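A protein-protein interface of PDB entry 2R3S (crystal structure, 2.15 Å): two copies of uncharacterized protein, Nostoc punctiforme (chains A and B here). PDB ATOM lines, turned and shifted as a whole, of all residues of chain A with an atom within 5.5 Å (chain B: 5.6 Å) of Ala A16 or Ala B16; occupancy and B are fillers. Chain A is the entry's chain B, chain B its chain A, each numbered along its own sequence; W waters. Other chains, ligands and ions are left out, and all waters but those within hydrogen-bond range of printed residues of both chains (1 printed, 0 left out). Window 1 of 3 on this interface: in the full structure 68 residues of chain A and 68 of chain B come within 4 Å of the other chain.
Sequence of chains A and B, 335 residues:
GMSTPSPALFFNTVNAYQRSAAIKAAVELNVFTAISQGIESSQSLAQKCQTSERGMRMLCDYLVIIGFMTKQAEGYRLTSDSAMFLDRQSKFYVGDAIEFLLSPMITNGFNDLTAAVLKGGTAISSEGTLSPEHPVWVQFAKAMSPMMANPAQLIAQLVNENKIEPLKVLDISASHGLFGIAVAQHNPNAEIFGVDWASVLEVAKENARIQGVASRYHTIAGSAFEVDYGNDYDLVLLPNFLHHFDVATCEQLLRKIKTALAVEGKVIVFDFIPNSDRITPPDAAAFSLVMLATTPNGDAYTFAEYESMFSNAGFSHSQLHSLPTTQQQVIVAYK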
ATOM      1  N   PHE A  11     -16.558   6.624  -7.268  1.00  0.00           N
ATOM      2  CA  PHE A  11     -17.744   5.749  -7.173  1.00  0.00           C
ATOM      3  C   PHE A  11     -18.794   5.975  -8.272  1.00  0.00           C
ATOM      4  O   PHE A  11     -19.433   5.032  -8.742  1.00  0.00           O
ATOM      5  CB  PHE A  11     -18.347   5.838  -5.758  1.00  0.00           C
ATOM      6  CG  PHE A  11     -17.477   5.205  -4.690  1.00  0.00           C
ATOM      7  CD1 PHE A  11     -17.187   3.845  -4.724  1.00  0.00           C
ATOM      8  CD2 PHE A  11     -16.937   5.961  -3.662  1.00  0.00           C
ATOM      9  CE1 PHE A  11     -16.372   3.253  -3.745  1.00  0.00           C
ATOM     10  CE2 PHE A  11     -16.141   5.372  -2.668  1.00  0.00           C
ATOM     11  CZ  PHE A  11     -15.857   4.014  -2.721  1.00  0.00           C
ATOM     12  N   ASN A  12     -18.994   7.209  -8.703  1.00  0.00           N
ATOM     13  CA  ASN A  12     -19.953   7.443  -9.796  1.00  0.00           C
ATOM     14  C   ASN A  12     -19.418   6.933 -11.144  1.00  0.00           C
ATOM     15  O   ASN A  12     -20.181   6.468 -11.984  1.00  0.00           O
ATOM     16  CB  ASN A  12     -20.323   8.924  -9.899  1.00  0.00           C
ATOM     17  CG  ASN A  12     -21.024   9.464  -8.630  1.00  0.00           C
ATOM     18  OD1 ASN A  12     -21.666   8.723  -7.868  1.00  0.00           O
ATOM     19  ND2 ASN A  12     -20.889  10.771  -8.406  1.00  0.00           N
ATOM     20  N   THR A  13     -18.114   7.053 -11.361  1.00  0.00           N
ATOM     21  CA  THR A  13     -17.447   6.505 -12.549  1.00  0.00           C
ATOM     22  C   THR A  13     -17.528   4.981 -12.526  1.00  0.00           C
ATOM     23  O   THR A  13     -17.891   4.355 -13.533  1.00  0.00           O
ATOM     24  CB  THR A  13     -15.984   6.996 -12.620  1.00  0.00           C
ATOM     25  OG1 THR A  13     -15.997   8.418 -12.541  1.00  0.00           O
ATOM     26  CG2 THR A  13     -15.288   6.570 -13.894  1.00  0.00           C
ATOM     27  N   VAL A  14     -17.246   4.388 -11.370  1.00  0.00           N
ATOM     28  CA  VAL A  14     -17.296   2.933 -11.212  1.00  0.00           C
ATOM     29  C   VAL A  14     -18.678   2.405 -11.568  1.00  0.00           C
ATOM     30  O   VAL A  14     -18.795   1.391 -12.225  1.00  0.00           O
ATOM     31  CB  VAL A  14     -16.898   2.475  -9.756  1.00  0.00           C
ATOM     32  CG1 VAL A  14     -17.256   1.008  -9.498  1.00  0.00           C
ATOM     33  CG2 VAL A  14     -15.373   2.702  -9.477  1.00  0.00           C
ATOM     34  N   ASN A  15     -19.726   3.093 -11.148  1.00  0.00           N
ATOM     35  CA  ASN A  15     -21.101   2.614 -11.394  1.00  0.00           C
ATOM     36  C   ASN A  15     -21.758   3.167 -12.659  1.00  0.00           C
ATOM     37  O   ASN A  15     -22.921   2.908 -12.908  1.00  0.00           O
ATOM     38  CB  ASN A  15     -21.987   2.969 -10.200  1.00  0.00           C
ATOM     39  CG  ASN A  15     -21.709   2.093  -8.989  1.00  0.00           C
ATOM     40  OD1 ASN A  15     -21.205   0.963  -9.087  1.00  0.00           O
ATOM     41  ND2 ASN A  15     -22.028   2.616  -7.848  1.00  0.00           N
ATOM     42  N   ALA A  16     -21.017   3.969 -13.408  1.00  0.00           N
ATOM     43  CA  ALA A  16     -21.484   4.588 -14.663  1.00  0.00           C
ATOM     44  C   ALA A  16     -22.128   3.577 -15.636  1.00  0.00           C
ATOM     45  O   ALA A  16     -23.043   3.939 -16.375  1.00  0.00           O
ATOM     46  CB  ALA A  16     -20.304   5.350 -15.357  1.00  0.00           C
ATOM     47  N   TYR A  17     -21.661   2.329 -15.630  1.00  0.00           N
ATOM     48  CA  TYR A  17     -22.190   1.300 -16.532  1.00  0.00           C
ATOM     49  C   TYR A  17     -23.698   1.136 -16.307  1.00  0.00           C
ATOM     50  O   TYR A  17     -24.438   0.757 -17.214  1.00  0.00           O
ATOM     51  CB  TYR A  17     -21.469  -0.055 -16.339  1.00  0.00           C
ATOM     52  CG  TYR A  17     -21.815  -0.738 -15.024  1.00  0.00           C
ATOM     53  CD1 TYR A  17     -21.119  -0.445 -13.858  1.00  0.00           C
ATOM     54  CD2 TYR A  17     -22.870  -1.651 -14.950  1.00  0.00           C
ATOM     55  CE1 TYR A  17     -21.478  -1.025 -12.654  1.00  0.00           C
ATOM     56  CE2 TYR A  17     -23.223  -2.240 -13.762  1.00  0.00           C
ATOM     57  CZ  TYR A  17     -22.535  -1.921 -12.613  1.00  0.00           C
ATOM     58  OH  TYR A  17     -22.924  -2.501 -11.430  1.00  0.00           O
ATOM     59  N   GLN A  18     -24.146   1.397 -15.085  1.00  0.00           N
ATOM     60  CA  GLN A  18     -25.552   1.287 -14.771  1.00  0.00           C
ATOM     61  C   GLN A  18     -26.419   2.261 -15.584  1.00  0.00           C
ATOM     62  O   GLN A  18     -27.533   1.941 -15.896  1.00  0.00           O
ATOM     63  CB  GLN A  18     -25.758   1.480 -13.277  1.00  0.00           C
ATOM     64  CG  GLN A  18     -25.050   0.425 -12.403  1.00  0.00           C
ATOM     65  CD  GLN A  18     -25.283   0.659 -10.930  1.00  0.00           C
ATOM     66  OE1 GLN A  18     -25.771   1.705 -10.547  1.00  0.00           O
ATOM     67  NE2 GLN A  18     -24.915  -0.312 -10.093  1.00  0.00           N
ATOM     68  N   ARG A  19     -25.871   3.414 -15.944  1.00  0.00           N
ATOM     69  CA  ARG A  19     -26.592   4.447 -16.684  1.00  0.00           C
ATOM     70  C   ARG A  19     -26.823   3.996 -18.092  1.00  0.00           C
ATOM     71  O   ARG A  19     -27.863   4.260 -18.659  1.00  0.00           O
ATOM     72  CB  ARG A  19     -25.823   5.782 -16.734  1.00  0.00           C
ATOM     73  CG  ARG A  19     -25.592   6.495 -15.395  1.00  0.00           C
ATOM     74  CD  ARG A  19     -24.698   7.769 -15.603  1.00  0.00           C
ATOM     75  NE  ARG A  19     -24.039   8.193 -14.373  1.00  0.00           N
ATOM     76  N   SER A  20     -25.827   3.329 -18.646  1.00  0.00           N
ATOM     77  CA  SER A  20     -25.917   2.744 -19.958  1.00  0.00           C
ATOM     78  C   SER A  20     -26.970   1.667 -19.973  1.00  0.00           C
ATOM     79  O   SER A  20     -27.709   1.608 -20.922  1.00  0.00           O
ATOM     80  CB  SER A  20     -24.576   2.177 -20.411  1.00  0.00           C
ATOM     81  OG  SER A  20     -23.619   3.211 -20.415  1.00  0.00           O
ATOM     82  N   PHE B  11     -26.228  10.360 -25.566  1.00  0.00           N
ATOM     83  CA  PHE B  11     -25.039   9.697 -26.076  1.00  0.00           C
ATOM     84  C   PHE B  11     -24.002   9.514 -24.968  1.00  0.00           C
ATOM     85  O   PHE B  11     -23.345   8.476 -24.905  1.00  0.00           O
ATOM     86  CB  PHE B  11     -24.458  10.424 -27.304  1.00  0.00           C
ATOM     87  CG  PHE B  11     -25.287  10.256 -28.567  1.00  0.00           C
ATOM     88  CD1 PHE B  11     -25.463   9.018 -29.136  1.00  0.00           C
ATOM     89  CD2 PHE B  11     -25.875  11.337 -29.178  1.00  0.00           C
ATOM     90  CE1 PHE B  11     -26.215   8.862 -30.270  1.00  0.00           C
ATOM     91  CE2 PHE B  11     -26.617  11.179 -30.315  1.00  0.00           C
ATOM     92  CZ  PHE B  11     -26.788   9.939 -30.861  1.00  0.00           C
ATOM     93  N   ASN B  12     -23.881  10.483 -24.071  1.00  0.00           N
ATOM     94  CA  ASN B  12     -22.965  10.313 -22.927  1.00  0.00           C
ATOM     95  C   ASN B  12     -23.414   9.200 -22.015  1.00  0.00           C
ATOM     96  O   ASN B  12     -22.589   8.459 -21.483  1.00  0.00           O
ATOM     97  CB  ASN B  12     -22.813  11.616 -22.123  1.00  0.00           C
ATOM     98  CG  ASN B  12     -22.202  12.729 -22.954  1.00  0.00           C
ATOM     99  OD1 ASN B  12     -21.416  12.478 -23.881  1.00  0.00           O
ATOM    100  ND2 ASN B  12     -22.569  13.969 -22.636  1.00  0.00           N
ATOM    101  N   THR B  13     -24.723   9.083 -21.851  1.00  0.00           N
ATOM    102  CA  THR B  13     -25.327   7.986 -21.084  1.00  0.00           C
ATOM    103  C   THR B  13     -25.169   6.654 -21.774  1.00  0.00           C
ATOM    104  O   THR B  13     -24.746   5.693 -21.158  1.00  0.00           O
ATOM    105  CB  THR B  13     -26.776   8.283 -20.772  1.00  0.00           C
ATOM    106  OG1 THR B  13     -26.827   9.564 -20.127  1.00  0.00           O
ATOM    107  CG2 THR B  13     -27.333   7.260 -19.840  1.00  0.00           C
ATOM    108  N   VAL B  14     -25.437   6.585 -23.066  1.00  0.00           N
ATOM    109  CA  VAL B  14     -25.225   5.329 -23.791  1.00  0.00           C
ATOM    110  C   VAL B  14     -23.798   4.836 -23.568  1.00  0.00           C
ATOM    111  O   VAL B  14     -23.599   3.665 -23.250  1.00  0.00           O
ATOM    112  CB  VAL B  14     -25.571   5.448 -25.298  1.00  0.00           C
ATOM    113  CG1 VAL B  14     -25.162   4.159 -26.084  1.00  0.00           C
ATOM    114  CG2 VAL B  14     -27.062   5.707 -25.460  1.00  0.00           C
ATOM    115  N   ASN B  15     -22.812   5.732 -23.709  1.00  0.00           N
ATOM    116  CA  ASN B  15     -21.383   5.373 -23.603  1.00  0.00           C
ATOM    117  C   ASN B  15     -20.757   5.380 -22.212  1.00  0.00           C
ATOM    118  O   ASN B  15     -19.557   5.111 -22.073  1.00  0.00           O
ATOM    119  CB  ASN B  15     -20.547   6.301 -24.496  1.00  0.00           C
ATOM    120  CG  ASN B  15     -20.830   6.105 -25.947  1.00  0.00           C
ATOM    121  OD1 ASN B  15     -21.359   5.074 -26.371  1.00  0.00           O
ATOM    122  ND2 ASN B  15     -20.466   7.076 -26.725  1.00  0.00           N
ATOM    123  N   ALA B  16     -21.571   5.642 -21.188  1.00  0.00           N
ATOM    124  CA  ALA B  16     -21.121   5.708 -19.797  1.00  0.00           C
ATOM    125  C   ALA B  16     -20.386   4.466 -19.311  1.00  0.00           C
ATOM    126  O   ALA B  16     -19.521   4.597 -18.446  1.00  0.00           O
ATOM    127  CB  ALA B  16     -22.337   6.068 -18.812  1.00  0.00           C
ATOM    128  N   TYR B  17     -20.731   3.279 -19.830  1.00  0.00           N
ATOM    129  CA  TYR B  17     -20.040   2.040 -19.493  1.00  0.00           C
ATOM    130  C   TYR B  17     -18.509   2.151 -19.734  1.00  0.00           C
ATOM    131  O   TYR B  17     -17.742   1.487 -19.081  1.00  0.00           O
ATOM    132  CB  TYR B  17     -20.635   0.802 -20.226  1.00  0.00           C
ATOM    133  CG  TYR B  17     -20.294   0.787 -21.676  1.00  0.00           C
ATOM    134  CD1 TYR B  17     -21.053   1.513 -22.596  1.00  0.00           C
ATOM    135  CD2 TYR B  17     -19.172   0.115 -22.131  1.00  0.00           C
ATOM    136  CE1 TYR B  17     -20.696   1.564 -23.921  1.00  0.00           C
ATOM    137  CE2 TYR B  17     -18.804   0.151 -23.475  1.00  0.00           C
ATOM    138  CZ  TYR B  17     -19.559   0.874 -24.362  1.00  0.00           C
ATOM    139  OH  TYR B  17     -19.201   0.906 -25.689  1.00  0.00           O
ATOM    140  N   GLN B  18     -18.071   3.033 -20.633  1.00  0.00           N
ATOM    141  CA  GLN B  18     -16.650   3.200 -20.959  1.00  0.00           C
ATOM    142  C   GLN B  18     -15.851   3.815 -19.801  1.00  0.00           C
ATOM    143  O   GLN B  18     -14.666   3.538 -19.620  1.00  0.00           O
ATOM    144  CB  GLN B  18     -16.515   4.037 -22.252  1.00  0.00           C
ATOM    145  CG  GLN B  18     -17.101   3.305 -23.483  1.00  0.00           C
ATOM    146  CD  GLN B  18     -17.174   4.137 -24.768  1.00  0.00           C
ATOM    147  OE1 GLN B  18     -16.790   5.308 -24.799  1.00  0.00           O
ATOM    148  NE2 GLN B  18     -17.664   3.517 -25.842  1.00  0.00           N
ATOM    149  N   ARG B  19     -16.512   4.662 -19.025  1.00  0.00           N
ATOM    150  CA  ARG B  19     -15.908   5.294 -17.896  1.00  0.00           C
ATOM    151  C   ARG B  19     -15.582   4.243 -16.868  1.00  0.00           C
ATOM    152  O   ARG B  19     -14.505   4.269 -16.291  1.00  0.00           O
ATOM    153  CB  ARG B  19     -16.872   6.289 -17.269  1.00  0.00           C
ATOM    154  CG  ARG B  19     -17.290   7.438 -18.143  1.00  0.00           C
ATOM    155  CD  ARG B  19     -18.209   8.339 -17.326  1.00  0.00           C
ATOM    156  NE  ARG B  19     -17.919   9.733 -17.576  1.00  0.00           N
ATOM    157  CZ  ARG B  19     -18.639  10.520 -18.358  1.00  0.00           C
ATOM    158  NH1 ARG B  19     -19.729  10.048 -18.963  1.00  0.00           N
ATOM    159  NH2 ARG B  19     -18.261  11.788 -18.525  1.00  0.00           N
ATOM    160  N   SER B  20     -16.541   3.343 -16.635  1.00  0.00           N
ATOM    161  CA  SER B  20     -16.383   2.228 -15.705  1.00  0.00           C
ATOM    162  C   SER B  20     -15.191   1.347 -16.093  1.00  0.00           C
ATOM    163  O   SER B  20     -14.374   0.987 -15.248  1.00  0.00           O
ATOM    164  CB  SER B  20     -17.655   1.347 -15.624  1.00  0.00           C
ATOM    165  OG  SER B  20     -18.805   2.065 -15.195  1.00  0.00           O
HETATM  166  O   HOH W   1     -17.011   9.812 -14.865  1.00  0.00           O
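The backbone carbonyl oxygen of Thr B13 sits at hydrogen-bond distance from the side-chain hydroxyl of Ser A20 (2.8 Å). The backbone carbonyl oxygen of Val B14 sits at hydrogen-bond distance from the side-chain hydroxyl of Ser A20 (2.9 Å). The backbone NH (N) of Ala B16 sits at hydrogen-bond distance from the side-chain hydroxyl (OG) of Ser A20 (3.3 Å). The backbone NH of Tyr B17 lies within hydrogen-bond range of the side-chain hydroxyl of Ser A20. The side-chain hydroxyl (OG) of Ser B20 is in hydrogen-bond range of the backbone carbonyl oxygen (O) of Thr A13, 3.0 Å away. The backbone carbonyl oxygen (O) of Val A14 sits at hydrogen-bond distance from the side-chain hydroxyl (OG) of Ser B20. The backbone NH (N) of Ala A16 lies within hydrogen-bond range of the side-chain hydroxyl (OG) of Ser B20, 3.4 Å away. N of Tyr A17 sits at hydrogen-bond distance from OG of Ser B20, 2.9 Å away.
OH of Tyr B17 sits at hydrogen-bond distance from NE2 of Gln B18, at 3.0 Å. OH of Tyr A17 lies within hydrogen-bond range of NE2 of Gln A18 (3.2 Å).
Among the printed residues, merely in contact across the chains: Thr A13 with Arg B19 (3.4 Å), Ala A16 with Ala B16 (3.3 Å), Tyr A17 with Tyr B17 (3.7 Å) and Arg A19 with Thr B13 (3.3 Å).
Of chain B, only Ala B16 and Ser B20 come within 4 Å of Ala A16. Printed residues of chain A within 4 Å of Ala B16: Ala A16 (3.3 Å) and Ser A20 (3.3 Å). Of the printed residues of chain B, Arg A19 touches Thr B13. Of the printed residues of chain A, Thr B13 touches Arg A19 and Ser A20. Printed residues of chain A within 4 Å of Arg B19: Thr A13 (3.4 Å). Of the printed residues of chain B, Ser A20 touches Thr B13, Val B14, Ala B16 and Tyr B17. Of the printed residues of chain A, Val B14 touches Ser A20 (2.9 Å). Asn A15 touches none of the printed residues of chain B. Asn B12 touches none of the printed residues of chain A.
Of the 10 printed residues of chain B, 6 touch a printed residue of chain A. Hydrophobic or aromatic side chains of chain A within 4 Å of the printed part of chain B: Ala A16 and Tyr A17. Among the printed residues, 12 pairs touch across the chains. Among the printed residues, no Asp or Glu carboxylate lies within 4 Å of a Lys or Arg side-chain nitrogen of the other chain.
Val A14 touches Ser B20, and with the chains exchanged Ser A20 touches Val B14. Ala B16 touches its own counterpart, Ala A16. Ala A16 touches Ser B20, and with the chains exchanged Ser A20 touches Ala B16. Tyr A17 touches Ser B20, and with the chains exchanged Ser A20 touches Tyr B17.
Water W1 lies within hydrogen-bond range of the guanidinium group (NE) of Arg B19 (2.9 Å) and the side-chain hydroxyl (OG1) of Thr A13 (2.9 Å).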
